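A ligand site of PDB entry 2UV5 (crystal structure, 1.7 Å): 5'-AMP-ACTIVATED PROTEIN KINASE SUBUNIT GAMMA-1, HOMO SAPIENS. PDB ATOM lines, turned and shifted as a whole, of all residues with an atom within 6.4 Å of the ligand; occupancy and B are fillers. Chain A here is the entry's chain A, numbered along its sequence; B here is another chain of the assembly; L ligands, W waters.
An oxygen (O7) of the ligand lies within hydrogen-bond range of the side-chain hydroxyl of Ser 143 (2.5 Å).
OD2 of Asp 144 sits at hydrogen-bond distance from O3 of the ligand (2.6 Å).
The side-chain hydroxyl (OG1) of Thr 27 is in hydrogen-bond range of an oxygen (O3) of the ligand, 2.7 Å away.
O1 of the ligand is in hydrogen-bond range of N of Ala 32, 2.9 Å away.
N1 of the ligand lies within hydrogen-bond range of O of Ala 32 (3.2 Å).
OG of Ser 53 of chain A sits at hydrogen-bond distance from O6 of the ligand.
A nitrogen (N1) of the ligand is in hydrogen-bond range of the backbone carbonyl oxygen of Ala 54 (3.0 Å).
O8 of the ligand lies close to OG of Ser 141 (3.3 Å).
The side-chain hydroxyl of Ser 141 sits close to the backbone NH of Ser 143 (3.5 Å).
OG of Ser 143 is in hydrogen-bond range of NZ of Lys 70 of chain B (2.7 Å).
OD2 of Asp 144 lies within hydrogen-bond range of N of Ser 141, 2.9 Å away.
N of Thr 27 sits at hydrogen-bond distance from O of Ile 139, at 2.8 Å.
Ile 31 touches the ligand (CA to O1, 3.4 Å).
CG1 of Val 52 touches C1 of the ligand (3.3 Å).
Pro 56 touches the ligand.
O of Ile 139 touches O3 of the ligand, at 3.5 Å.
Within 4 Å of the ligand: Thr 27, Ile 31, Ala 32, Val 52, Ser 53 of chain A, Ala 54, Pro 56, Ile 139, Ser 141, Ser 143 and Asp 144.
Water W7 lies within hydrogen-bond range of O8 of the ligand, OG of Ser 53 of chain A and NH2 of Arg 126.
Water W10 lies within hydrogen-bond range of an oxygen (O8) of the ligand (2.7 Å), the backbone NH of Leu 142 (3.1 Å) and the backbone NH of Ser 143 (3.3 Å).
Water W9 lies within hydrogen-bond range of O7 of the ligand, NZ of Lys 70 of chain B and OG of Ser 143.
Water W6 lies within hydrogen-bond range of N of Ala 54 (2.8 Å), N3 of the ligand (2.8 Å) and OG of Ser 53 of chain A (3.1 Å).
Water W8 lies within hydrogen-bond range of OG of Ser 53 of chain A (2.8 Å) and O6 of the ligand (2.9 Å).
Water W13 lies within hydrogen-bond range of OG1 of Thr 27 (2.8 Å), O of Gly 26 (3.3 Å) and O2 of the ligand (3.5 Å).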
ATOM      1  N   GLY A  26     -26.821  -3.695 -17.822  1.00  0.00           N
ATOM      2  CA  GLY A  26     -27.098  -3.199 -16.466  1.00  0.00           C
ATOM      3  C   GLY A  26     -25.934  -3.386 -15.491  1.00  0.00           C
ATOM      4  O   GLY A  26     -24.935  -4.045 -15.824  1.00  0.00           O
ATOM      5  N   THR A  27     -26.074  -2.802 -14.297  1.00  0.00           N
ATOM      6  CA  THR A  27     -25.116  -2.962 -13.214  1.00  0.00           C
ATOM      7  C   THR A  27     -25.808  -3.705 -12.113  1.00  0.00           C
ATOM      8  O   THR A  27     -26.877  -3.298 -11.695  1.00  0.00           O
ATOM      9  CB  THR A  27     -24.626  -1.611 -12.677  1.00  0.00           C
ATOM     10  OG1 THR A  27     -24.035  -0.896 -13.756  1.00  0.00           O
ATOM     11  CG2 THR A  27     -23.569  -1.806 -11.512  1.00  0.00           C
ATOM     12  N   ALA A  29     -23.951  -5.074  -9.237  1.00  0.00           N
ATOM     13  CA  ALA A  29     -23.092  -5.109  -8.049  1.00  0.00           C
ATOM     14  C   ALA A  29     -22.829  -3.694  -7.560  1.00  0.00           C
ATOM     15  O   ALA A  29     -22.751  -2.736  -8.362  1.00  0.00           O
ATOM     16  CB  ALA A  29     -21.778  -5.795  -8.389  1.00  0.00           C
ATOM     17  N   ASN A  30     -22.698  -3.543  -6.240  1.00  0.00           N
ATOM     18  CA  ASN A  30     -22.218  -2.309  -5.637  1.00  0.00           C
ATOM     19  C   ASN A  30     -23.128  -1.102  -5.834  1.00  0.00           C
ATOM     20  O   ASN A  30     -22.670   0.040  -5.737  1.00  0.00           O
ATOM     21  CB  ASN A  30     -20.804  -2.009  -6.116  1.00  0.00           C
ATOM     22  CG  ASN A  30     -19.821  -3.098  -5.719  1.00  0.00           C
ATOM     23  OD1 ASN A  30     -20.077  -3.844  -4.758  1.00  0.00           O
ATOM     24  ND2 ASN A  30     -18.671  -3.127  -6.390  1.00  0.00           N
ATOM     25  N   ILE A  31     -24.423  -1.381  -6.050  1.00  0.00           N
ATOM     26  CA  ILE A  31     -25.429  -0.327  -6.186  1.00  0.00           C
ATOM     27  C   ILE A  31     -25.560   0.524  -4.914  1.00  0.00           C
ATOM     28  O   ILE A  31     -25.740   0.009  -3.789  1.00  0.00           O
ATOM     29  CB  ILE A  31     -26.828  -0.909  -6.540  1.00  0.00           C
ATOM     30  CG1 ILE A  31     -26.814  -1.670  -7.883  1.00  0.00           C
ATOM     31  CG2 ILE A  31     -27.858   0.188  -6.543  1.00  0.00           C
ATOM     32  CD1 ILE A  31     -26.195  -0.933  -9.055  1.00  0.00           C
ATOM     33  N   ALA A  32     -25.510   1.835  -5.116  1.00  0.00           N
ATOM     34  CA  ALA A  32     -25.745   2.783  -4.013  1.00  0.00           C
ATOM     35  C   ALA A  32     -27.224   3.135  -3.985  1.00  0.00           C
ATOM     36  O   ALA A  32     -27.847   3.381  -5.035  1.00  0.00           O
ATOM     37  CB  ALA A  32     -24.893   4.035  -4.187  1.00  0.00           C
ATOM     38  N   MET A  33     -27.789   3.184  -2.791  1.00  0.00           N
ATOM     39  CA  MET A  33     -29.229   3.381  -2.628  1.00  0.00           C
ATOM     40  C   MET A  33     -29.483   3.984  -1.263  1.00  0.00           C
ATOM     41  O   MET A  33     -28.612   3.955  -0.383  1.00  0.00           O
ATOM     42  CB  MET A  33     -29.994   2.054  -2.784  1.00  0.00           C
ATOM     43  CG  MET A  33     -29.502   0.965  -1.887  1.00  0.00           C
ATOM     44  SD  MET A  33     -30.122  -0.638  -2.407  1.00  0.00           S
ATOM     45  CE  MET A  33     -31.693  -0.621  -1.594  1.00  0.00           C
ATOM     46  N   HIS A  50     -19.294  10.166  -4.064  1.00  0.00           N
ATOM     47  CA  HIS A  50     -19.312   8.807  -4.609  1.00  0.00           C
ATOM     48  C   HIS A  50     -19.471   8.769  -6.129  1.00  0.00           C
ATOM     49  O   HIS A  50     -19.197   7.730  -6.736  1.00  0.00           O
ATOM     50  CB  HIS A  50     -20.400   7.951  -3.954  1.00  0.00           C
ATOM     51  CG  HIS A  50     -20.249   6.474  -4.211  1.00  0.00           C
ATOM     52  ND1 HIS A  50     -19.192   5.735  -3.709  1.00  0.00           N
ATOM     53  CD2 HIS A  50     -21.015   5.608  -4.911  1.00  0.00           C
ATOM     54  CE1 HIS A  50     -19.312   4.482  -4.110  1.00  0.00           C
ATOM     55  NE2 HIS A  50     -20.411   4.377  -4.836  1.00  0.00           N
ATOM     56  N   VAL A  52     -22.268   9.033  -8.377  1.00  0.00           N
ATOM     57  CA  VAL A  52     -23.401   8.263  -8.917  1.00  0.00           C
ATOM     58  C   VAL A  52     -24.411   9.330  -9.324  1.00  0.00           C
ATOM     59  O   VAL A  52     -24.486  10.330  -8.652  1.00  0.00           O
ATOM     60  CB  VAL A  52     -24.228   7.505  -7.862  1.00  0.00           C
ATOM     61  CG1 VAL A  52     -24.608   6.124  -8.355  1.00  0.00           C
ATOM     62  CG2 VAL A  52     -23.614   7.542  -6.519  1.00  0.00           C
ATOM     63  N   SER A  53     -25.232   9.098 -10.350  1.00  0.00           N
ATOM     64  CA  SER A  53     -26.200  10.139 -10.687  1.00  0.00           C
ATOM     65  C   SER A  53     -27.624   9.937 -10.156  1.00  0.00           C
ATOM     66  O   SER A  53     -28.397  10.882 -10.144  1.00  0.00           O
ATOM     67  CB  SER A  53     -26.211  10.426 -12.190  1.00  0.00           C
ATOM     68  OG  SER A  53     -26.147   9.229 -12.922  1.00  0.00           O
ATOM     69  N   ALA A  54     -27.953   8.737  -9.677  1.00  0.00           N
ATOM     70  CA  ALA A  54     -29.311   8.466  -9.160  1.00  0.00           C
ATOM     71  C   ALA A  54     -29.314   7.285  -8.202  1.00  0.00           C
ATOM     72  O   ALA A  54     -28.519   6.360  -8.340  1.00  0.00           O
ATOM     73  CB  ALA A  54     -30.299   8.250 -10.288  1.00  0.00           C
ATOM     74  N   LEU A  55     -30.194   7.353  -7.219  1.00  0.00           N
ATOM     75  CA  LEU A  55     -30.207   6.422  -6.116  1.00  0.00           C
ATOM     76  C   LEU A  55     -31.595   5.831  -5.918  1.00  0.00           C
ATOM     77  O   LEU A  55     -32.531   6.587  -5.681  1.00  0.00           O
ATOM     78  CB  LEU A  55     -29.859   7.165  -4.841  1.00  0.00           C
ATOM     79  CG  LEU A  55     -28.509   7.864  -4.786  1.00  0.00           C
ATOM     80  CD1 LEU A  55     -28.575   9.004  -3.772  1.00  0.00           C
ATOM     81  CD2 LEU A  55     -27.417   6.824  -4.470  1.00  0.00           C
ATOM     82  N   PRO A  56     -31.721   4.504  -6.049  1.00  0.00           N
ATOM     83  CA  PRO A  56     -32.991   3.872  -5.712  1.00  0.00           C
ATOM     84  C   PRO A  56     -33.346   4.247  -4.277  1.00  0.00           C
ATOM     85  O   PRO A  56     -32.429   4.370  -3.428  1.00  0.00           O
ATOM     86  CB  PRO A  56     -32.684   2.389  -5.848  1.00  0.00           C
ATOM     87  CG  PRO A  56     -31.594   2.327  -6.850  1.00  0.00           C
ATOM     88  CD  PRO A  56     -30.735   3.535  -6.561  1.00  0.00           C
ATOM     89  N   HIS A 125     -34.050   8.485 -17.299  1.00  0.00           N
ATOM     90  CA  HIS A 125     -32.713   8.106 -17.771  1.00  0.00           C
ATOM     91  C   HIS A 125     -32.200   6.788 -17.190  1.00  0.00           C
ATOM     92  O   HIS A 125     -31.087   6.364 -17.485  1.00  0.00           O
ATOM     93  CB  HIS A 125     -31.744   9.236 -17.413  1.00  0.00           C
ATOM     94  CG  HIS A 125     -31.982  10.491 -18.183  1.00  0.00           C
ATOM     95  ND1 HIS A 125     -31.119  11.566 -18.128  1.00  0.00           N
ATOM     96  CD2 HIS A 125     -32.974  10.849 -19.040  1.00  0.00           C
ATOM     97  CE1 HIS A 125     -31.590  12.531 -18.911  1.00  0.00           C
ATOM     98  NE2 HIS A 125     -32.706  12.121 -19.473  1.00  0.00           N
ATOM     99  N   ARG A 126     -33.014   6.164 -16.343  1.00  0.00           N
ATOM    100  CA  ARG A 126     -32.694   4.848 -15.809  1.00  0.00           C
ATOM    101  C   ARG A 126     -33.909   4.173 -15.183  1.00  0.00           C
ATOM    102  O   ARG A 126     -34.913   4.821 -14.842  1.00  0.00           O
ATOM    103  CB  ARG A 126     -31.581   4.913 -14.752  1.00  0.00           C
ATOM    104  CG  ARG A 126     -31.996   5.449 -13.395  1.00  0.00           C
ATOM    105  CD  ARG A 126     -32.169   6.954 -13.347  1.00  0.00           C
ATOM    106  NE  ARG A 126     -30.964   7.680 -13.688  1.00  0.00           N
ATOM    107  CZ  ARG A 126     -30.869   9.007 -13.721  1.00  0.00           C
ATOM    108  NH1 ARG A 126     -31.911   9.763 -13.386  1.00  0.00           N
ATOM    109  NH2 ARG A 126     -29.718   9.569 -14.065  1.00  0.00           N
ATOM    110  N   ILE A 139     -29.438  -1.813 -11.771  1.00  0.00           N
ATOM    111  CA  ILE A 139     -29.815  -0.607 -12.468  1.00  0.00           C
ATOM    112  C   ILE A 139     -29.469  -0.716 -13.944  1.00  0.00           C
ATOM    113  O   ILE A 139     -28.383  -1.210 -14.327  1.00  0.00           O
ATOM    114  CB  ILE A 139     -29.046   0.642 -11.936  1.00  0.00           C
ATOM    115  CG1 ILE A 139     -29.262   0.859 -10.445  1.00  0.00           C
ATOM    116  CG2 ILE A 139     -29.525   1.899 -12.683  1.00  0.00           C
ATOM    117  CD1 ILE A 139     -30.521   1.621 -10.091  1.00  0.00           C
ATOM    118  N   VAL A 140     -30.373  -0.169 -14.765  1.00  0.00           N
ATOM    119  CA  VAL A 140     -30.125  -0.002 -16.209  1.00  0.00           C
ATOM    120  C   VAL A 140     -30.314   1.463 -16.565  1.00  0.00           C
ATOM    121  O   VAL A 140     -31.402   2.019 -16.382  1.00  0.00           O
ATOM    122  CB  VAL A 140     -31.099  -0.817 -17.068  1.00  0.00           C
ATOM    123  CG1 VAL A 140     -30.864  -0.505 -18.579  1.00  0.00           C
ATOM    124  CG2 VAL A 140     -30.985  -2.321 -16.777  1.00  0.00           C
ATOM    125  N   SER A 141     -29.254   2.096 -17.027  1.00  0.00           N
ATOM    126  CA  SER A 141     -29.304   3.506 -17.418  1.00  0.00           C
ATOM    127  C   SER A 141     -29.076   3.639 -18.923  1.00  0.00           C
ATOM    128  O   SER A 141     -28.762   2.652 -19.637  1.00  0.00           O
ATOM    129  CB  SER A 141     -28.213   4.278 -16.670  1.00  0.00           C
ATOM    130  OG  SER A 141     -26.959   3.848 -17.138  1.00  0.00           O
ATOM    131  N   LEU A 142     -29.178   4.861 -19.414  1.00  0.00           N
ATOM    132  CA  LEU A 142     -28.986   5.095 -20.842  1.00  0.00           C
ATOM    133  C   LEU A 142     -27.611   4.569 -21.272  1.00  0.00           C
ATOM    134  O   LEU A 142     -27.462   3.935 -22.335  1.00  0.00           O
ATOM    135  CB  LEU A 142     -29.096   6.585 -21.175  1.00  0.00           C
ATOM    136  CG  LEU A 142     -30.360   7.361 -20.727  1.00  0.00           C
ATOM    137  CD1 LEU A 142     -30.305   8.842 -21.197  1.00  0.00           C
ATOM    138  CD2 LEU A 142     -31.615   6.664 -21.237  1.00  0.00           C
ATOM    139  N   SER A 143     -26.601   4.828 -20.444  1.00  0.00           N
ATOM    140  CA  SER A 143     -25.234   4.377 -20.762  1.00  0.00           C
ATOM    141  C   SER A 143     -25.157   2.869 -21.073  1.00  0.00           C
ATOM    142  O   SER A 143     -24.521   2.434 -22.040  1.00  0.00           O
ATOM    143  CB  SER A 143     -24.289   4.778 -19.651  1.00  0.00           C
ATOM    144  OG  SER A 143     -24.292   6.190 -19.542  1.00  0.00           O
ATOM    145  N   ASP A 144     -25.830   2.079 -20.243  1.00  0.00           N
ATOM    146  CA  ASP A 144     -25.852   0.631 -20.395  1.00  0.00           C
ATOM    147  C   ASP A 144     -26.536   0.215 -21.701  1.00  0.00           C
ATOM    148  O   ASP A 144     -26.085  -0.739 -22.356  1.00  0.00           O
ATOM    149  CB  ASP A 144     -26.622   0.007 -19.245  1.00  0.00           C
ATOM    150  CG  ASP A 144     -25.986   0.278 -17.887  1.00  0.00           C
ATOM    151  OD1 ASP A 144     -24.766   0.135 -17.786  1.00  0.00           O
ATOM    152  OD2 ASP A 144     -26.701   0.640 -16.918  1.00  0.00           O
ATOM    153  N   GLN A 147     -24.146   1.085 -24.667  1.00  0.00           N
ATOM    154  CA  GLN A 147     -23.018   0.127 -24.705  1.00  0.00           C
ATOM    155  C   GLN A 147     -23.365  -1.133 -25.475  1.00  0.00           C
ATOM    156  O   GLN A 147     -22.544  -1.655 -26.230  1.00  0.00           O
ATOM    157  CB  GLN A 147     -22.613  -0.321 -23.290  1.00  0.00           C
ATOM    158  CG  GLN A 147     -21.687   0.620 -22.561  1.00  0.00           C
ATOM    159  CD  GLN A 147     -21.628   0.319 -21.058  1.00  0.00           C
ATOM    160  OE1 GLN A 147     -21.759  -0.843 -20.639  1.00  0.00           O
ATOM    161  NE2 GLN A 147     -21.436   1.362 -20.251  1.00  0.00           N
ATOM    162  N   SER B  53     -21.770  12.542 -21.473  1.00  0.00           N
ATOM    163  CA  SER B  53     -23.202  12.303 -21.635  1.00  0.00           C
ATOM    164  C   SER B  53     -23.937  13.234 -22.603  1.00  0.00           C
ATOM    165  O   SER B  53     -25.047  12.907 -23.007  1.00  0.00           O
ATOM    166  CB  SER B  53     -23.917  12.259 -20.282  1.00  0.00           C
ATOM    167  OG  SER B  53     -23.442  13.275 -19.439  1.00  0.00           O
ATOM    168  N   LYS B  70     -27.297  11.415 -24.711  1.00  0.00           N
ATOM    169  CA  LYS B  70     -27.590   9.977 -24.732  1.00  0.00           C
ATOM    170  C   LYS B  70     -29.108   9.725 -24.865  1.00  0.00           C
ATOM    171  O   LYS B  70     -29.552   8.789 -25.576  1.00  0.00           O
ATOM    172  CB  LYS B  70     -27.002   9.321 -23.495  1.00  0.00           C
ATOM    173  CG  LYS B  70     -25.491   9.250 -23.489  1.00  0.00           C
ATOM    174  CD  LYS B  70     -24.930   8.564 -22.221  1.00  0.00           C
ATOM    175  CE  LYS B  70     -23.459   8.209 -22.324  1.00  0.00           C
ATOM    176  NZ  LYS B  70     -22.907   7.981 -20.947  1.00  0.00           N
HETATM  177  O1  LIG L   1     -25.193   2.602  -7.888  1.00  0.00           O
HETATM  178  C1  LIG L   1     -25.987   3.183  -8.563  1.00  0.00           C
HETATM  179  N1  LIG L   1     -27.064   3.802  -8.078  1.00  0.00           N
HETATM  180  C2  LIG L   1     -25.793   3.234  -9.983  1.00  0.00           C
HETATM  181  C3  LIG L   1     -24.823   2.568 -10.709  1.00  0.00           C
HETATM  182  N2  LIG L   1     -23.863   1.706 -10.299  1.00  0.00           N
HETATM  183  N3  LIG L   1     -26.574   4.021 -10.805  1.00  0.00           N
HETATM  184  C4  LIG L   1     -26.082   3.806 -12.018  1.00  0.00           C
HETATM  185  N4  LIG L   1     -25.036   2.917 -12.017  1.00  0.00           N
HETATM  186  C5  LIG L   1     -24.267   2.503 -13.176  1.00  0.00           C
HETATM  187  C6  LIG L   1     -25.109   2.371 -14.454  1.00  0.00           C
HETATM  188  C7  LIG L   1     -24.022   2.579 -15.526  1.00  0.00           C
HETATM  189  O2  LIG L   1     -23.364   1.367 -15.882  1.00  0.00           O
HETATM  190  O3  LIG L   1     -25.733   1.095 -14.537  1.00  0.00           O
HETATM  191  O4  LIG L   1     -23.345   3.576 -13.460  1.00  0.00           O
HETATM  192  C8  LIG L   1     -23.026   3.565 -14.857  1.00  0.00           C
HETATM  193  C9  LIG L   1     -23.113   4.987 -15.359  1.00  0.00           C
HETATM  194  O5  LIG L   1     -24.504   5.336 -15.342  1.00  0.00           O
HETATM  195  P1  LIG L   1     -24.963   6.779 -15.779  1.00  0.00           P
HETATM  196  O6  LIG L   1     -24.415   7.730 -14.770  1.00  0.00           O
HETATM  197  O7  LIG L   1     -24.334   7.090 -17.170  1.00  0.00           O
HETATM  198  O8  LIG L   1     -26.494   6.895 -15.826  1.00  0.00           O
HETATM  199  O   HOH W   1     -24.319   6.907 -12.161  1.00  0.00           O
HETATM  200  O   HOH W   2     -21.215   3.111 -17.838  1.00  0.00           O
HETATM  201  O   HOH W   3     -21.282   1.179 -11.517  1.00  0.00           O
HETATM  202  O   HOH W   4     -22.671   3.747  -7.428  1.00  0.00           O
HETATM  203  O   HOH W   5     -28.185   6.429 -13.765  1.00  0.00           O
HETATM  204  O   HOH W   6     -27.170   6.709 -11.479  1.00  0.00           O
HETATM  205  O   HOH W   7     -27.148   9.458 -15.855  1.00  0.00           O
HETATM  206  O   HOH W   8     -25.048  10.567 -15.080  1.00  0.00           O
HETATM  207  O   HOH W   9     -24.580   9.505 -18.571  1.00  0.00           O
HETATM  208  O   HOH W  10     -27.482   7.164 -18.346  1.00  0.00           O
HETATM  209  O   HOH W  11     -21.491   7.045 -17.584  1.00  0.00           O
HETATM  210  O   HOH W  12     -22.313   5.452 -11.742  1.00  0.00           O
HETATM  211  O   HOH W  13     -22.434  -1.969 -15.789  1.00  0.00           O
HETATM  212  O   HOH W  14     -21.023   0.496 -14.014  1.00  0.00           O
